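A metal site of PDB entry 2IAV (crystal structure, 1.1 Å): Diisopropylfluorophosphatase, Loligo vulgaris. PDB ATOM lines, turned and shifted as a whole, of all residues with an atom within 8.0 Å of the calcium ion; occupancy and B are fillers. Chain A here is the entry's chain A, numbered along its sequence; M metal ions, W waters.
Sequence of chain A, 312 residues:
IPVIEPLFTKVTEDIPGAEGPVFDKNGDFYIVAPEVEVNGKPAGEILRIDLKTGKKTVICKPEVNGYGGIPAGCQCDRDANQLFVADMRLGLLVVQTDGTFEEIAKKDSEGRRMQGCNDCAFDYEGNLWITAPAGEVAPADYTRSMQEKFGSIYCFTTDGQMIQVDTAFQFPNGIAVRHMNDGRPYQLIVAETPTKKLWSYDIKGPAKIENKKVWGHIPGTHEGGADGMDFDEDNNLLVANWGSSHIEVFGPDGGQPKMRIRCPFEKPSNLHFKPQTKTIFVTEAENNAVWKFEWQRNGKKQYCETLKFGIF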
ATOM      1  N   GLU A  19     -18.045  17.402   0.074  1.00  0.00           N
ATOM      2  CA  GLU A  19     -19.363  17.024  -0.395  1.00  0.00           C
ATOM      3  C   GLU A  19     -19.634  17.696  -1.730  1.00  0.00           C
ATOM      4  O   GLU A  19     -18.781  18.483  -2.243  1.00  0.00           O
ATOM      5  CB  GLU A  19     -20.448  17.399   0.662  1.00  0.00           C
ATOM      6  CG  GLU A  19     -21.162  16.212   1.423  1.00  0.00           C
ATOM      7  CD  GLU A  19     -22.239  15.515   0.627  1.00  0.00           C
ATOM      8  OE1 GLU A  19     -22.309  15.701  -0.602  1.00  0.00           O
ATOM      9  OE2 GLU A  19     -23.079  14.866   1.280  1.00  0.00           O
ATOM     10  N   GLY A  20     -20.820  17.408  -2.279  1.00  0.00           N
ATOM     11  CA  GLY A  20     -21.321  18.102  -3.456  1.00  0.00           C
ATOM     12  C   GLY A  20     -20.410  18.266  -4.651  1.00  0.00           C
ATOM     13  O   GLY A  20     -20.335  19.393  -5.191  1.00  0.00           O
ATOM     14  N   PRO A  21     -19.708  17.230  -5.083  1.00  0.00           N
ATOM     15  CA  PRO A  21     -18.841  17.393  -6.280  1.00  0.00           C
ATOM     16  C   PRO A  21     -19.686  17.718  -7.501  1.00  0.00           C
ATOM     17  O   PRO A  21     -20.768  17.136  -7.725  1.00  0.00           O
ATOM     18  CB  PRO A  21     -18.191  15.998  -6.423  1.00  0.00           C
ATOM     19  CG  PRO A  21     -19.210  15.039  -5.769  1.00  0.00           C
ATOM     20  CD  PRO A  21     -19.827  15.820  -4.649  1.00  0.00           C
ATOM     21  N   VAL A  22     -19.168  18.642  -8.336  1.00  0.00           N
ATOM     22  CA  VAL A  22     -19.954  19.042  -9.491  1.00  0.00           C
ATOM     23  C   VAL A  22     -19.006  19.635 -10.537  1.00  0.00           C
ATOM     24  O   VAL A  22     -17.950  20.251 -10.213  1.00  0.00           O
ATOM     25  CB  VAL A  22     -21.023  20.073  -9.060  1.00  0.00           C
ATOM     26  CG1 VAL A  22     -20.429  21.389  -8.531  1.00  0.00           C
ATOM     27  CG2 VAL A  22     -22.034  20.342 -10.181  1.00  0.00           C
ATOM     28  N   PHE A  23     -19.332  19.440 -11.807  1.00  0.00           N
ATOM     29  CA  PHE A  23     -18.661  20.116 -12.926  1.00  0.00           C
ATOM     30  C   PHE A  23     -19.576  21.193 -13.492  1.00  0.00           C
ATOM     31  O   PHE A  23     -20.801  21.013 -13.576  1.00  0.00           O
ATOM     32  CB  PHE A  23     -18.314  19.106 -14.043  1.00  0.00           C
ATOM     33  CG  PHE A  23     -17.129  18.248 -13.706  1.00  0.00           C
ATOM     34  CD1 PHE A  23     -15.826  18.674 -13.986  1.00  0.00           C
ATOM     35  CD2 PHE A  23     -17.279  17.020 -13.089  1.00  0.00           C
ATOM     36  CE1 PHE A  23     -14.708  17.874 -13.683  1.00  0.00           C
ATOM     37  CE2 PHE A  23     -16.161  16.238 -12.743  1.00  0.00           C
ATOM     38  CZ  PHE A  23     -14.875  16.664 -13.041  1.00  0.00           C
ATOM     39  N   CYS A  74     -24.702  20.133  -4.788  1.00  0.00           N
ATOM     40  CA  CYS A  74     -24.696  21.060  -5.932  1.00  0.00           C
ATOM     41  C   CYS A  74     -25.254  20.425  -7.202  1.00  0.00           C
ATOM     42  O   CYS A  74     -25.127  19.190  -7.404  1.00  0.00           O
ATOM     43  CB  CYS A  74     -23.248  21.496  -6.280  1.00  0.00           C
ATOM     44  SG  CYS A  74     -22.314  22.180  -4.876  1.00  0.00           S
ATOM     45  N   GLN A  75     -25.767  21.298  -8.056  1.00  0.00           N
ATOM     46  CA  GLN A  75     -26.071  21.030  -9.458  1.00  0.00           C
ATOM     47  C   GLN A  75     -25.644  22.256 -10.283  1.00  0.00           C
ATOM     48  O   GLN A  75     -25.747  23.389  -9.786  1.00  0.00           O
ATOM     49  CB  GLN A  75     -27.553  20.798  -9.690  1.00  0.00           C
ATOM     50  CG  GLN A  75     -28.121  19.526  -9.127  1.00  0.00           C
ATOM     51  CD  GLN A  75     -27.707  18.298  -9.906  1.00  0.00           C
ATOM     52  OE1 GLN A  75     -26.593  17.756  -9.633  1.00  0.00           O
ATOM     53  NE2 GLN A  75     -28.477  17.891 -10.831  1.00  0.00           N
ATOM     54  N   ASP A 119     -29.110  18.021  -0.789  1.00  0.00           N
ATOM     55  CA  ASP A 119     -28.660  17.708  -2.137  1.00  0.00           C
ATOM     56  C   ASP A 119     -29.796  18.010  -3.109  1.00  0.00           C
ATOM     57  O   ASP A 119     -30.943  18.310  -2.700  1.00  0.00           O
ATOM     58  CB  ASP A 119     -28.193  16.240  -2.240  1.00  0.00           C
ATOM     59  CG  ASP A 119     -27.108  15.976  -3.267  1.00  0.00           C
ATOM     60  OD1 ASP A 119     -26.834  16.865  -4.109  1.00  0.00           O
ATOM     61  OD2 ASP A 119     -26.523  14.849  -3.234  1.00  0.00           O
ATOM     62  N   CYS A 120     -29.477  18.014  -4.386  1.00  0.00           N
ATOM     63  CA  CYS A 120     -30.463  18.380  -5.392  1.00  0.00           C
ATOM     64  C   CYS A 120     -30.155  17.708  -6.740  1.00  0.00           C
ATOM     65  O   CYS A 120     -29.001  17.310  -6.985  1.00  0.00           O
ATOM     66  CB  CYS A 120     -30.611  19.903  -5.490  1.00  0.00           C
ATOM     67  SG  CYS A 120     -29.162  20.849  -5.901  1.00  0.00           S
ATOM     68  N   ILE A 175     -30.425  12.380  -4.091  1.00  0.00           N
ATOM     69  CA  ILE A 175     -31.630  12.447  -4.915  1.00  0.00           C
ATOM     70  C   ILE A 175     -31.203  12.390  -6.360  1.00  0.00           C
ATOM     71  O   ILE A 175     -30.103  12.887  -6.708  1.00  0.00           O
ATOM     72  CB  ILE A 175     -32.420  13.734  -4.548  1.00  0.00           C
ATOM     73  CG1 ILE A 175     -33.794  13.803  -5.278  1.00  0.00           C
ATOM     74  CG2 ILE A 175     -31.588  14.977  -4.756  1.00  0.00           C
ATOM     75  CD1 ILE A 175     -34.735  14.810  -4.598  1.00  0.00           C
ATOM     76  N   GLY A 228     -25.000  10.460  -1.307  1.00  0.00           N
ATOM     77  CA  GLY A 228     -25.236  10.963  -2.653  1.00  0.00           C
ATOM     78  C   GLY A 228     -25.334   9.891  -3.698  1.00  0.00           C
ATOM     79  O   GLY A 228     -24.905   8.731  -3.504  1.00  0.00           O
ATOM     80  N   MET A 229     -25.894  10.261  -4.848  1.00  0.00           N
ATOM     81  CA  MET A 229     -26.139   9.279  -5.919  1.00  0.00           C
ATOM     82  C   MET A 229     -26.123   9.957  -7.300  1.00  0.00           C
ATOM     83  O   MET A 229     -26.314  11.190  -7.432  1.00  0.00           O
ATOM     84  CB  MET A 229     -27.532   8.640  -5.750  1.00  0.00           C
ATOM     85  CG  MET A 229     -28.711   9.584  -5.847  1.00  0.00           C
ATOM     86  SD  MET A 229     -30.312   8.887  -5.570  1.00  0.00           S
ATOM     87  CE  MET A 229     -29.773   7.712  -4.234  1.00  0.00           C
ATOM     88  N   ASP A 230     -25.948   9.126  -8.328  1.00  0.00           N
ATOM     89  CA  ASP A 230     -26.084   9.573  -9.728  1.00  0.00           C
ATOM     90  C   ASP A 230     -26.275   8.370 -10.612  1.00  0.00           C
ATOM     91  O   ASP A 230     -25.831   7.250 -10.295  1.00  0.00           O
ATOM     92  CB  ASP A 230     -24.838  10.328 -10.227  1.00  0.00           C
ATOM     93  CG  ASP A 230     -24.842  11.894  -9.940  1.00  0.00           C
ATOM     94  OD1 ASP A 230     -25.872  12.491 -10.246  1.00  0.00           O
ATOM     95  OD2 ASP A 230     -23.785  12.391  -9.564  1.00  0.00           O
ATOM     96  N   PHE A 231     -26.880   8.619 -11.763  1.00  0.00           N
ATOM     97  CA  PHE A 231     -27.067   7.591 -12.777  1.00  0.00           C
ATOM     98  C   PHE A 231     -25.905   7.532 -13.763  1.00  0.00           C
ATOM     99  O   PHE A 231     -25.312   8.569 -14.144  1.00  0.00           O
ATOM    100  CB  PHE A 231     -28.317   7.877 -13.596  1.00  0.00           C
ATOM    101  CG  PHE A 231     -29.607   7.550 -12.881  1.00  0.00           C
ATOM    102  CD1 PHE A 231     -29.981   6.225 -12.708  1.00  0.00           C
ATOM    103  CD2 PHE A 231     -30.452   8.571 -12.413  1.00  0.00           C
ATOM    104  CE1 PHE A 231     -31.163   5.910 -12.105  1.00  0.00           C
ATOM    105  CE2 PHE A 231     -31.654   8.224 -11.768  1.00  0.00           C
ATOM    106  CZ  PHE A 231     -32.010   6.894 -11.619  1.00  0.00           C
ATOM    107  N   LEU A 238     -25.758   4.689  -9.028  1.00  0.00           N
ATOM    108  CA  LEU A 238     -24.621   4.528  -8.127  1.00  0.00           C
ATOM    109  C   LEU A 238     -24.847   5.360  -6.874  1.00  0.00           C
ATOM    110  O   LEU A 238     -25.178   6.573  -6.991  1.00  0.00           O
ATOM    111  CB  LEU A 238     -23.317   4.925  -8.829  1.00  0.00           C
ATOM    112  CG  LEU A 238     -22.859   3.962  -9.953  1.00  0.00           C
ATOM    113  CD1 LEU A 238     -23.527   4.344 -11.285  1.00  0.00           C
ATOM    114  CD2 LEU A 238     -21.363   3.895 -10.136  1.00  0.00           C
ATOM    115  N   ASN A 270     -20.422  11.305  -1.577  1.00  0.00           N
ATOM    116  CA  ASN A 270     -21.100  11.753  -2.759  1.00  0.00           C
ATOM    117  C   ASN A 270     -20.182  11.491  -3.948  1.00  0.00           C
ATOM    118  O   ASN A 270     -19.019  11.067  -3.808  1.00  0.00           O
ATOM    119  CB  ASN A 270     -21.501  13.243  -2.646  1.00  0.00           C
ATOM    120  CG  ASN A 270     -22.815  13.573  -3.336  1.00  0.00           C
ATOM    121  OD1 ASN A 270     -23.546  14.504  -2.857  1.00  0.00           O
ATOM    122  ND2 ASN A 270     -23.160  12.880  -4.335  1.00  0.00           N
ATOM    123  N   LEU A 271     -20.719  11.701  -5.125  1.00  0.00           N
ATOM    124  CA  LEU A 271     -20.040  11.314  -6.349  1.00  0.00           C
ATOM    125  C   LEU A 271     -20.561  12.163  -7.520  1.00  0.00           C
ATOM    126  O   LEU A 271     -21.641  12.758  -7.479  1.00  0.00           O
ATOM    127  CB  LEU A 271     -20.096   9.806  -6.599  1.00  0.00           C
ATOM    128  CG  LEU A 271     -21.451   9.175  -6.682  1.00  0.00           C
ATOM    129  CD1 LEU A 271     -22.066   9.313  -7.952  1.00  0.00           C
ATOM    130  CD2 LEU A 271     -21.301   7.622  -6.312  1.00  0.00           C
ATOM    131  N   HIS A 272     -19.763  12.184  -8.582  1.00  0.00           N
ATOM    132  CA  HIS A 272     -20.156  12.913  -9.788  1.00  0.00           C
ATOM    133  C   HIS A 272     -19.265  12.476 -10.934  1.00  0.00           C
ATOM    134  O   HIS A 272     -18.044  12.328 -10.763  1.00  0.00           O
ATOM    135  CB  HIS A 272     -19.992  14.409  -9.621  1.00  0.00           C
ATOM    136  CG  HIS A 272     -21.026  15.184 -10.361  1.00  0.00           C
ATOM    137  ND1 HIS A 272     -22.355  15.212  -9.989  1.00  0.00           N
ATOM    138  CD2 HIS A 272     -20.921  16.029 -11.418  1.00  0.00           C
ATOM    139  CE1 HIS A 272     -23.016  15.992 -10.811  1.00  0.00           C
ATOM    140  NE2 HIS A 272     -22.171  16.563 -11.645  1.00  0.00           N
ATOM    141  N   PHE A 273     -19.880  12.271 -12.098  1.00  0.00           N
ATOM    142  CA  PHE A 273     -19.123  11.911 -13.284  1.00  0.00           C
ATOM    143  C   PHE A 273     -18.513  13.167 -13.896  1.00  0.00           C
ATOM    144  O   PHE A 273     -19.120  14.221 -13.911  1.00  0.00           O
ATOM    145  CB  PHE A 273     -20.021  11.265 -14.376  1.00  0.00           C
ATOM    146  CG  PHE A 273     -20.398   9.832 -14.098  1.00  0.00           C
ATOM    147  CD1 PHE A 273     -21.473   9.523 -13.271  1.00  0.00           C
ATOM    148  CD2 PHE A 273     -19.712   8.805 -14.720  1.00  0.00           C
ATOM    149  CE1 PHE A 273     -21.834   8.203 -13.069  1.00  0.00           C
ATOM    150  CE2 PHE A 273     -20.070   7.479 -14.540  1.00  0.00           C
ATOM    151  CZ  PHE A 273     -21.139   7.165 -13.724  1.00  0.00           C
ATOM    152  N   ILE A 280     -15.472   8.846 -12.228  1.00  0.00           N
ATOM    153  CA  ILE A 280     -16.334   9.291 -11.158  1.00  0.00           C
ATOM    154  C   ILE A 280     -15.448   9.865 -10.069  1.00  0.00           C
ATOM    155  O   ILE A 280     -14.500   9.223  -9.598  1.00  0.00           O
ATOM    156  CB  ILE A 280     -17.139   8.098 -10.605  1.00  0.00           C
ATOM    157  CG1 ILE A 280     -18.052   7.508 -11.690  1.00  0.00           C
ATOM    158  CG2 ILE A 280     -17.958   8.573  -9.378  1.00  0.00           C
ATOM    159  CD1 ILE A 280     -18.877   6.368 -11.190  1.00  0.00           C
ATOM    160  N   PHE A 281     -15.736  11.112  -9.722  1.00  0.00           N
ATOM    161  CA  PHE A 281     -15.138  11.790  -8.610  1.00  0.00           C
ATOM    162  C   PHE A 281     -15.942  11.481  -7.344  1.00  0.00           C
ATOM    163  O   PHE A 281     -17.173  11.613  -7.341  1.00  0.00           O
ATOM    164  CB  PHE A 281     -15.060  13.306  -8.885  1.00  0.00           C
ATOM    165  CG  PHE A 281     -14.009  13.645  -9.910  1.00  0.00           C
ATOM    166  CD1 PHE A 281     -14.183  13.305 -11.251  1.00  0.00           C
ATOM    167  CD2 PHE A 281     -12.796  14.218  -9.528  1.00  0.00           C
ATOM    168  CE1 PHE A 281     -13.162  13.557 -12.185  1.00  0.00           C
ATOM    169  CE2 PHE A 281     -11.780  14.444 -10.493  1.00  0.00           C
ATOM    170  CZ  PHE A 281     -11.986  14.140 -11.765  1.00  0.00           C
ATOM    171  N   GLN A 302     -25.914  15.239 -17.184  1.00  0.00           N
ATOM    172  CA  GLN A 302     -26.616  16.157 -16.292  1.00  0.00           C
ATOM    173  C   GLN A 302     -27.362  17.205 -17.118  1.00  0.00           C
ATOM    174  O   GLN A 302     -27.094  17.398 -18.309  1.00  0.00           O
ATOM    175  CB  GLN A 302     -25.600  16.841 -15.363  1.00  0.00           C
ATOM    176  CG  GLN A 302     -24.918  15.884 -14.364  1.00  0.00           C
ATOM    177  CD  GLN A 302     -25.721  15.766 -13.084  1.00  0.00           C
ATOM    178  OE1 GLN A 302     -26.367  14.696 -12.838  1.00  0.00           O
ATOM    179  NE2 GLN A 302     -25.726  16.771 -12.289  1.00  0.00           N
HETATM  180 CA    CA M   1     -23.371  14.022  -8.199  1.00  0.00          CA
HETATM  181  O   HOH W   1     -22.734  15.606  -6.881  1.00  0.00           O
HETATM  182  O   HOH W   2     -24.612  13.240  -6.539  1.00  0.00           O
HETATM  183  O   HOH W   3     -25.380  14.859  -8.930  1.00  0.00           O
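Water W3 lies within hydrogen-bond range of OD1 of Asp 230 (2.8 Å) and OE1 of Gln 75 (3.2 Å). Water W2 bridges the side-chain amide nitrogen (ND2) of Asn 270 and the backbone carbonyl oxygen (O) of Met 229.
Three residues have an atom within 4 Å of the calcium ion: Asp 230, Leu 271 and His 272. The nearest printed residue that does not touch the calcium ion is Asn 270 (4.03 Å).
The backbone carbonyl oxygen (O) of His 272 sits at hydrogen-bond distance from the backbone NH (N) of Phe 281 (2.8 Å). A ring nitrogen (ND1) of His 272 lies close to the backbone carbonyl oxygen (O) of Pro 21 (3.4 Å). OE1 of Gln 302 sits close to OD1 of Asp 230, at 3.4 Å. N of Leu 238 is in hydrogen-bond range of O of Asp 230 (2.9 Å).
The calcium ion is bound by water W1 (2.2 Å). The calcium ion is bound by OD2 of Asp 230, at 2.2 Å. Water W2 binds the calcium ion (2.2 Å). The calcium ion is bound by O of Leu 271 (2.3 Å). The calcium ion is bound by water W3, at 2.3 Å. The calcium ion is bound by a ring nitrogen (ND1) of His 272 (2.4 Å). The calcium ion has six donor atoms within binding distance.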
